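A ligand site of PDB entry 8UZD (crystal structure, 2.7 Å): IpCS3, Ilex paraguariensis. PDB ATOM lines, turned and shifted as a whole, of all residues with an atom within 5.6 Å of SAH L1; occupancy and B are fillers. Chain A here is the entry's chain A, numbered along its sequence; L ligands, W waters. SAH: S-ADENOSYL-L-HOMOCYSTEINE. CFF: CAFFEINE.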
ATOM      1  N   SER A  27      14.845 -31.175 -35.941  1.00  0.00           N
ATOM      2  CA  SER A  27      13.701 -30.293 -36.044  1.00  0.00           C
ATOM      3  C   SER A  27      12.579 -30.943 -36.848  1.00  0.00           C
ATOM      4  O   SER A  27      11.396 -30.795 -36.509  1.00  0.00           O
ATOM      5  CB  SER A  27      14.090 -28.958 -36.626  1.00  0.00           C
ATOM      6  OG  SER A  27      12.963 -28.106 -36.706  1.00  0.00           O
ATOM      7  N   THR A  31       8.699 -32.210 -35.432  1.00  0.00           N
ATOM      8  CA  THR A  31       7.471 -31.735 -36.041  1.00  0.00           C
ATOM      9  C   THR A  31       6.658 -32.900 -36.582  1.00  0.00           C
ATOM     10  O   THR A  31       5.427 -32.895 -36.489  1.00  0.00           O
ATOM     11  CB  THR A  31       7.734 -30.582 -37.024  1.00  0.00           C
ATOM     12  OG1 THR A  31       8.938 -30.938 -37.695  1.00  0.00           O
ATOM     13  CG2 THR A  31       7.990 -29.255 -36.336  1.00  0.00           C
ATOM     14  N   ASP A  60       0.103 -19.292 -32.675  1.00  0.00           N
ATOM     15  CA  ASP A  60       1.374 -19.989 -32.580  1.00  0.00           C
ATOM     16  C   ASP A  60       2.338 -19.134 -31.745  1.00  0.00           C
ATOM     17  O   ASP A  60       2.743 -18.062 -32.185  1.00  0.00           O
ATOM     18  CB  ASP A  60       1.939 -20.299 -33.976  1.00  0.00           C
ATOM     19  CG  ASP A  60       3.221 -21.125 -33.976  1.00  0.00           C
ATOM     20  OD1 ASP A  60       3.417 -21.927 -33.039  1.00  0.00           O
ATOM     21  OD2 ASP A  60       4.044 -20.956 -34.906  1.00  0.00           O
ATOM     22  N   LEU A  61       2.717 -19.610 -30.553  1.00  0.00           N
ATOM     23  CA  LEU A  61       3.599 -18.851 -29.682  1.00  0.00           C
ATOM     24  C   LEU A  61       5.077 -19.102 -30.025  1.00  0.00           C
ATOM     25  O   LEU A  61       5.540 -20.248 -29.990  1.00  0.00           O
ATOM     26  CB  LEU A  61       3.307 -19.206 -28.218  1.00  0.00           C
ATOM     27  CG  LEU A  61       1.835 -19.262 -27.832  1.00  0.00           C
ATOM     28  CD1 LEU A  61       1.668 -19.568 -26.340  1.00  0.00           C
ATOM     29  CD2 LEU A  61       1.109 -17.961 -28.192  1.00  0.00           C
ATOM     30  N   GLY A  62       5.807 -18.020 -30.330  1.00  0.00           N
ATOM     31  CA  GLY A  62       7.229 -18.082 -30.641  1.00  0.00           C
ATOM     32  C   GLY A  62       7.495 -18.781 -31.976  1.00  0.00           C
ATOM     33  O   GLY A  62       8.106 -19.845 -32.013  1.00  0.00           O
ATOM     34  N   CYS A  63       7.018 -18.163 -33.050  1.00  0.00           N
ATOM     35  CA  CYS A  63       6.926 -18.808 -34.351  1.00  0.00           C
ATOM     36  C   CYS A  63       8.267 -18.747 -35.086  1.00  0.00           C
ATOM     37  O   CYS A  63       8.488 -19.510 -36.029  1.00  0.00           O
ATOM     38  CB  CYS A  63       5.859 -18.137 -35.212  1.00  0.00           C
ATOM     39  SG  CYS A  63       6.130 -16.352 -35.428  1.00  0.00           S
ATOM     40  N   ALA A  64       9.161 -17.844 -34.653  1.00  0.00           N
ATOM     41  CA  ALA A  64      10.373 -17.492 -35.378  1.00  0.00           C
ATOM     42  C   ALA A  64      10.035 -17.147 -36.828  1.00  0.00           C
ATOM     43  O   ALA A  64       9.012 -16.515 -37.082  1.00  0.00           O
ATOM     44  CB  ALA A  64      11.404 -18.596 -35.289  1.00  0.00           C
ATOM     45  N   ASN A  68       8.274 -24.085 -39.820  1.00  0.00           N
ATOM     46  CA  ASN A  68       7.343 -24.704 -38.877  1.00  0.00           C
ATOM     47  C   ASN A  68       5.984 -23.975 -38.878  1.00  0.00           C
ATOM     48  O   ASN A  68       4.945 -24.633 -39.003  1.00  0.00           O
ATOM     49  CB  ASN A  68       7.964 -24.970 -37.502  1.00  0.00           C
ATOM     50  CG  ASN A  68       6.952 -25.318 -36.418  1.00  0.00           C
ATOM     51  OD1 ASN A  68       6.591 -26.475 -36.245  1.00  0.00           O
ATOM     52  ND2 ASN A  68       6.513 -24.321 -35.660  1.00  0.00           N
ATOM     53  N   PRO A  69       5.924 -22.626 -38.736  1.00  0.00           N
ATOM     54  CA  PRO A  69       4.656 -21.907 -38.831  1.00  0.00           C
ATOM     55  C   PRO A  69       3.840 -22.189 -40.087  1.00  0.00           C
ATOM     56  O   PRO A  69       2.621 -22.295 -40.020  1.00  0.00           O
ATOM     57  CB  PRO A  69       5.020 -20.423 -38.721  1.00  0.00           C
ATOM     58  CG  PRO A  69       6.532 -20.357 -38.787  1.00  0.00           C
ATOM     59  CD  PRO A  69       7.039 -21.729 -38.396  1.00  0.00           C
ATOM     60  N   ASN A  99       2.784 -15.316 -33.228  1.00  0.00           N
ATOM     61  CA  ASN A  99       3.456 -14.547 -32.178  1.00  0.00           C
ATOM     62  C   ASN A  99       4.949 -14.844 -32.147  1.00  0.00           C
ATOM     63  O   ASN A  99       5.354 -15.996 -32.275  1.00  0.00           O
ATOM     64  CB  ASN A  99       2.842 -14.804 -30.797  1.00  0.00           C
ATOM     65  CG  ASN A  99       3.777 -14.414 -29.675  1.00  0.00           C
ATOM     66  OD1 ASN A  99       4.411 -15.279 -29.077  1.00  0.00           O
ATOM     67  ND2 ASN A  99       3.915 -13.130 -29.393  1.00  0.00           N
ATOM     68  N   ASP A 100       5.743 -13.782 -31.955  1.00  0.00           N
ATOM     69  CA  ASP A 100       7.153 -13.825 -31.568  1.00  0.00           C
ATOM     70  C   ASP A 100       7.572 -12.446 -31.030  1.00  0.00           C
ATOM     71  O   ASP A 100       6.815 -11.479 -31.161  1.00  0.00           O
ATOM     72  CB  ASP A 100       8.045 -14.368 -32.689  1.00  0.00           C
ATOM     73  CG  ASP A 100       9.335 -14.993 -32.179  1.00  0.00           C
ATOM     74  OD1 ASP A 100      10.142 -14.256 -31.576  1.00  0.00           O
ATOM     75  OD2 ASP A 100       9.542 -16.219 -32.378  1.00  0.00           O
ATOM     76  N   LEU A 101       8.763 -12.351 -30.416  1.00  0.00           N
ATOM     77  CA  LEU A 101       9.258 -11.102 -29.860  1.00  0.00           C
ATOM     78  C   LEU A 101       9.422 -10.079 -30.981  1.00  0.00           C
ATOM     79  O   LEU A 101       9.642 -10.458 -32.132  1.00  0.00           O
ATOM     80  CB  LEU A 101      10.593 -11.353 -29.154  1.00  0.00           C
ATOM     81  CG  LEU A 101      10.474 -12.051 -27.795  1.00  0.00           C
ATOM     82  CD1 LEU A 101      11.813 -12.557 -27.314  1.00  0.00           C
ATOM     83  CD2 LEU A 101       9.817 -11.136 -26.771  1.00  0.00           C
ATOM     84  N   ASN A 104      11.930 -10.157 -34.062  1.00  0.00           N
ATOM     85  CA  ASN A 104      11.863 -11.332 -34.917  1.00  0.00           C
ATOM     86  C   ASN A 104      11.789 -10.837 -36.359  1.00  0.00           C
ATOM     87  O   ASN A 104      11.337  -9.716 -36.605  1.00  0.00           O
ATOM     88  CB  ASN A 104      10.706 -12.250 -34.511  1.00  0.00           C
ATOM     89  CG  ASN A 104      10.646 -13.539 -35.322  1.00  0.00           C
ATOM     90  OD1 ASN A 104      11.663 -14.160 -35.597  1.00  0.00           O
ATOM     91  ND2 ASN A 104       9.447 -13.940 -35.683  1.00  0.00           N
ATOM     92  N   GLY A 135       5.433  -9.284 -29.412  1.00  0.00           N
ATOM     93  CA  GLY A 135       5.271  -9.206 -27.973  1.00  0.00           C
ATOM     94  C   GLY A 135       5.773 -10.490 -27.301  1.00  0.00           C
ATOM     95  O   GLY A 135       6.125 -11.438 -27.986  1.00  0.00           O
ATOM     96  N   SER A 136       5.816 -10.485 -25.964  1.00  0.00           N
ATOM     97  CA  SER A 136       6.188 -11.662 -25.204  1.00  0.00           C
ATOM     98  C   SER A 136       4.931 -12.471 -24.852  1.00  0.00           C
ATOM     99  O   SER A 136       3.900 -11.911 -24.472  1.00  0.00           O
ATOM    100  CB  SER A 136       6.938 -11.284 -23.975  1.00  0.00           C
ATOM    101  OG  SER A 136       6.868 -12.322 -23.007  1.00  0.00           O
ATOM    102  N   PHE A 137       5.039 -13.808 -24.927  1.00  0.00           N
ATOM    103  CA  PHE A 137       3.888 -14.632 -24.564  1.00  0.00           C
ATOM    104  C   PHE A 137       3.717 -14.683 -23.039  1.00  0.00           C
ATOM    105  O   PHE A 137       2.748 -15.281 -22.573  1.00  0.00           O
ATOM    106  CB  PHE A 137       3.895 -16.003 -25.246  1.00  0.00           C
ATOM    107  CG  PHE A 137       5.194 -16.768 -25.204  1.00  0.00           C
ATOM    108  CD1 PHE A 137       5.796 -17.114 -23.995  1.00  0.00           C
ATOM    109  CD2 PHE A 137       5.814 -17.166 -26.386  1.00  0.00           C
ATOM    110  CE1 PHE A 137       7.001 -17.802 -23.978  1.00  0.00           C
ATOM    111  CE2 PHE A 137       7.024 -17.855 -26.360  1.00  0.00           C
ATOM    112  CZ  PHE A 137       7.605 -18.175 -25.150  1.00  0.00           C
ATOM    113  N   TYR A 138       4.644 -14.059 -22.292  1.00  0.00           N
ATOM    114  CA  TYR A 138       4.515 -13.927 -20.844  1.00  0.00           C
ATOM    115  C   TYR A 138       3.727 -12.663 -20.518  1.00  0.00           C
ATOM    116  O   TYR A 138       4.289 -11.650 -20.105  1.00  0.00           O
ATOM    117  CB  TYR A 138       5.870 -13.937 -20.142  1.00  0.00           C
ATOM    118  CG  TYR A 138       6.609 -15.239 -20.265  1.00  0.00           C
ATOM    119  CD1 TYR A 138       5.988 -16.432 -19.935  1.00  0.00           C
ATOM    120  CD2 TYR A 138       7.909 -15.283 -20.760  1.00  0.00           C
ATOM    121  CE1 TYR A 138       6.638 -17.657 -20.073  1.00  0.00           C
ATOM    122  CE2 TYR A 138       8.564 -16.491 -20.910  1.00  0.00           C
ATOM    123  CZ  TYR A 138       7.929 -17.682 -20.561  1.00  0.00           C
ATOM    124  OH  TYR A 138       8.570 -18.878 -20.704  1.00  0.00           O
ATOM    125  N   SER A 152       2.508 -24.259 -29.776  1.00  0.00           N
ATOM    126  CA  SER A 152       3.866 -23.793 -29.517  1.00  0.00           C
ATOM    127  C   SER A 152       4.852 -24.959 -29.590  1.00  0.00           C
ATOM    128  O   SER A 152       4.686 -25.979 -28.932  1.00  0.00           O
ATOM    129  CB  SER A 152       3.951 -23.106 -28.164  1.00  0.00           C
ATOM    130  OG  SER A 152       5.186 -22.413 -28.038  1.00  0.00           O
ATOM    131  N   CYS A 153       5.904 -24.755 -30.389  1.00  0.00           N
ATOM    132  CA  CYS A 153       6.920 -25.778 -30.580  1.00  0.00           C
ATOM    133  C   CYS A 153       8.309 -25.180 -30.350  1.00  0.00           C
ATOM    134  O   CYS A 153       8.766 -24.349 -31.118  1.00  0.00           O
ATOM    135  CB  CYS A 153       6.847 -26.331 -31.997  1.00  0.00           C
ATOM    136  SG  CYS A 153       7.985 -27.702 -32.301  1.00  0.00           S
ATOM    137  N   TYR A 154       8.945 -25.586 -29.242  1.00  0.00           N
ATOM    138  CA  TYR A 154      10.317 -25.221 -28.918  1.00  0.00           C
ATOM    139  C   TYR A 154      10.489 -23.739 -28.583  1.00  0.00           C
ATOM    140  O   TYR A 154      11.489 -23.123 -28.996  1.00  0.00           O
ATOM    141  CB  TYR A 154      11.280 -25.833 -29.946  1.00  0.00           C
ATOM    142  CG  TYR A 154      11.851 -27.142 -29.482  1.00  0.00           C
ATOM    143  CD1 TYR A 154      11.020 -28.246 -29.273  1.00  0.00           C
ATOM    144  CD2 TYR A 154      13.204 -27.290 -29.220  1.00  0.00           C
ATOM    145  CE1 TYR A 154      11.530 -29.460 -28.826  1.00  0.00           C
ATOM    146  CE2 TYR A 154      13.729 -28.488 -28.769  1.00  0.00           C
ATOM    147  CZ  TYR A 154      12.884 -29.572 -28.562  1.00  0.00           C
ATOM    148  OH  TYR A 154      13.381 -30.747 -28.094  1.00  0.00           O
ATOM    149  N   SER A 155       9.566 -23.175 -27.784  1.00  0.00           N
ATOM    150  CA  SER A 155       9.678 -21.769 -27.377  1.00  0.00           C
ATOM    151  C   SER A 155       9.597 -21.627 -25.863  1.00  0.00           C
ATOM    152  O   SER A 155      10.369 -20.894 -25.264  1.00  0.00           O
ATOM    153  CB  SER A 155       8.616 -20.921 -28.012  1.00  0.00           C
ATOM    154  OG  SER A 155       8.530 -21.156 -29.400  1.00  0.00           O
ATOM    155  N   TRP A 158      12.170 -21.201 -22.894  1.00  0.00           N
ATOM    156  CA  TRP A 158      12.932 -19.980 -22.684  1.00  0.00           C
ATOM    157  C   TRP A 158      12.262 -19.159 -21.581  1.00  0.00           C
ATOM    158  O   TRP A 158      11.058 -18.942 -21.633  1.00  0.00           O
ATOM    159  CB  TRP A 158      12.996 -19.156 -23.971  1.00  0.00           C
ATOM    160  CG  TRP A 158      13.766 -19.776 -25.079  1.00  0.00           C
ATOM    161  CD1 TRP A 158      13.282 -20.315 -26.234  1.00  0.00           C
ATOM    162  CD2 TRP A 158      15.195 -19.892 -25.160  1.00  0.00           C
ATOM    163  NE1 TRP A 158      14.302 -20.767 -27.019  1.00  0.00           N
ATOM    164  CE2 TRP A 158      15.496 -20.523 -26.384  1.00  0.00           C
ATOM    165  CE3 TRP A 158      16.249 -19.525 -24.306  1.00  0.00           C
ATOM    166  CZ2 TRP A 158      16.805 -20.776 -26.774  1.00  0.00           C
ATOM    167  CZ3 TRP A 158      17.542 -19.803 -24.690  1.00  0.00           C
ATOM    168  CH2 TRP A 158      17.810 -20.402 -25.917  1.00  0.00           C
ATOM    169  N   LEU A 159      13.055 -18.707 -20.617  1.00  0.00           N
ATOM    170  CA  LEU A 159      12.528 -18.011 -19.462  1.00  0.00           C
ATOM    171  C   LEU A 159      12.456 -16.514 -19.755  1.00  0.00           C
ATOM    172  O   LEU A 159      13.042 -16.033 -20.719  1.00  0.00           O
ATOM    173  CB  LEU A 159      13.415 -18.332 -18.253  1.00  0.00           C
ATOM    174  CG  LEU A 159      13.637 -19.815 -17.959  1.00  0.00           C
ATOM    175  CD1 LEU A 159      14.842 -20.005 -17.055  1.00  0.00           C
ATOM    176  CD2 LEU A 159      12.406 -20.463 -17.347  1.00  0.00           C
HETATM  177  N   SAH L   1       8.389 -22.549 -33.086  1.00  0.00           N
HETATM  178  CA  SAH L   1       9.435 -22.450 -34.162  1.00  0.00           C
HETATM  179  CB  SAH L   1      10.653 -21.645 -33.690  1.00  0.00           C
HETATM  180  CG  SAH L   1      11.167 -22.040 -32.325  1.00  0.00           C
HETATM  181  SD  SAH L   1      12.548 -21.005 -31.787  1.00  0.00           S
HETATM  182  C   SAH L   1       9.876 -23.844 -34.621  1.00  0.00           C
HETATM  183  O   SAH L   1      10.802 -23.934 -35.409  1.00  0.00           O
HETATM  184  OXT SAH L   1       9.362 -24.918 -34.270  1.00  0.00           O
HETATM  185  C5' SAH L   1      11.888 -20.228 -30.273  1.00  0.00           C
HETATM  186  C4' SAH L   1      11.342 -18.827 -30.505  1.00  0.00           C
HETATM  187  O4' SAH L   1      10.661 -18.342 -29.330  1.00  0.00           O
HETATM  188  C3' SAH L   1      12.398 -17.766 -30.847  1.00  0.00           C
HETATM  189  O3' SAH L   1      12.164 -17.241 -32.146  1.00  0.00           O
HETATM  190  C2' SAH L   1      12.248 -16.707 -29.750  1.00  0.00           C
HETATM  191  O2' SAH L   1      12.432 -15.389 -30.204  1.00  0.00           O
HETATM  192  C1' SAH L   1      10.816 -16.941 -29.297  1.00  0.00           C
HETATM  193  N9  SAH L   1      10.510 -16.457 -27.956  1.00  0.00           N
HETATM  194  C8  SAH L   1      11.245 -16.661 -26.807  1.00  0.00           C
HETATM  195  N7  SAH L   1      10.694 -16.133 -25.753  1.00  0.00           N
HETATM  196  C5  SAH L   1       9.518 -15.543 -26.212  1.00  0.00           C
HETATM  197  C6  SAH L   1       8.483 -14.827 -25.569  1.00  0.00           C
HETATM  198  N6  SAH L   1       8.459 -14.558 -24.269  1.00  0.00           N
HETATM  199  N1  SAH L   1       7.447 -14.404 -26.329  1.00  0.00           N
HETATM  200  C2  SAH L   1       7.471 -14.664 -27.641  1.00  0.00           C
HETATM  201  N3  SAH L   1       8.386 -15.321 -28.352  1.00  0.00           N
HETATM  202  C4  SAH L   1       9.402 -15.750 -27.570  1.00  0.00           C
HETATM  203  N1  CFF L   2      15.871 -24.532 -29.639  1.00  0.00           N
HETATM  204  C2  CFF L   2      16.092 -25.588 -30.547  1.00  0.00           C
HETATM  205  C10 CFF L   2      15.334 -23.265 -30.181  1.00  0.00           C
HETATM  206  C6  CFF L   2      16.104 -24.559 -28.246  1.00  0.00           C
HETATM  207  N3  CFF L   2      16.573 -26.779 -30.038  1.00  0.00           N
HETATM  208  O11 CFF L   2      15.865 -25.453 -31.742  1.00  0.00           O
HETATM  209  C12 CFF L   2      16.808 -27.905 -30.946  1.00  0.00           C
HETATM  210  C4  CFF L   2      16.815 -26.885 -28.690  1.00  0.00           C
HETATM  211  C5  CFF L   2      16.599 -25.830 -27.819  1.00  0.00           C
HETATM  212  N9  CFF L   2      17.286 -27.983 -28.033  1.00  0.00           N
HETATM  213  O13 CFF L   2      15.876 -23.590 -27.546  1.00  0.00           O
HETATM  214  N7  CFF L   2      16.960 -26.298 -26.548  1.00  0.00           N
HETATM  215  C8  CFF L   2      17.341 -27.600 -26.754  1.00  0.00           C
HETATM  216  C14 CFF L   2      16.899 -25.544 -25.295  1.00  0.00           C
HETATM  217  O   HOH W   1       5.760 -22.400 -31.940  1.00  0.00           O
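The backbone NH (N) of Phe 137 sits at hydrogen-bond distance from a nitrogen (N1) of SAH L1 (2.8 Å).
The backbone carbonyl oxygen of Cys 153 sits at hydrogen-bond distance from a nitrogen (N) of SAH L1, 2.7 Å away.
The backbone carbonyl oxygen (O) of Gly 62 lies within hydrogen-bond range of a nitrogen (N) of SAH L1.
The side-chain carboxylate (OD2) of Asp 100 sits at hydrogen-bond distance from an oxygen (O3') of SAH L1 (2.8 Å).
OG of Ser 136 lies within hydrogen-bond range of N6 of SAH L1 (3.0 Å).
An oxygen (O13) of CFF L2 sits close to the indole nitrogen (NE1) of Trp 158 (3.3 Å).
SG of Cys 153 sits close to OXT of SAH L1.
The side-chain amide nitrogen (ND2) of Asn 68 is in hydrogen-bond range of an oxygen (OXT) of SAH L1, at 3.2 Å.
ND2 of Asn 99 lies within hydrogen-bond range of O of Gly 135, at 3.1 Å.
The backbone carbonyl oxygen of Asn 99 sits at hydrogen-bond distance from the backbone NH of Gly 62 (2.8 Å).
O of Gly 62 is in hydrogen-bond range of OG of Ser 155, 3.0 Å away.
O of Asn 99 is in hydrogen-bond range of N of Cys 63.
OD2 of Asp 100 lies within hydrogen-bond range of N of Ala 64, at 2.8 Å.
The side-chain hydroxyl (OH) of Tyr 138 is in hydrogen-bond range of the backbone carbonyl oxygen (O) of Trp 158.
The backbone carbonyl oxygen (O) of Asp 100 lies within hydrogen-bond range of the backbone NH (N) of Gly 135, 3.1 Å away.
The backbone carbonyl oxygen (O) of Leu 61 sits at hydrogen-bond distance from the side-chain hydroxyl (OG) of Ser 155, 3.2 Å away.
A sulfur (SD) of SAH L1 sits close to the backbone carbonyl oxygen (O) of Tyr 154, 3.7 Å away.
Cys 63 touches SAH L1 (O to CA, 3.6 Å).
Ala 64 touches SAH L1.
Asn 99 touches SAH L1 (OD1 to C2, 3.4 Å).
Leu 101 touches SAH L1 (N to N3, 3.6 Å).
Gly 135 touches SAH L1.
Tyr 138 touches SAH L1 (CD2 to N6, 3.6 Å).
OG of Ser 155 touches O4' of SAH L1, at 3.5 Å.
Hydrophobic or aromatic side chains within 4 Å of SAH L1: Ala 64, Leu 101, Phe 137 and Tyr 138.
The nearest printed residue that does not touch SAH L1 is Trp 158 (4.1 Å).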
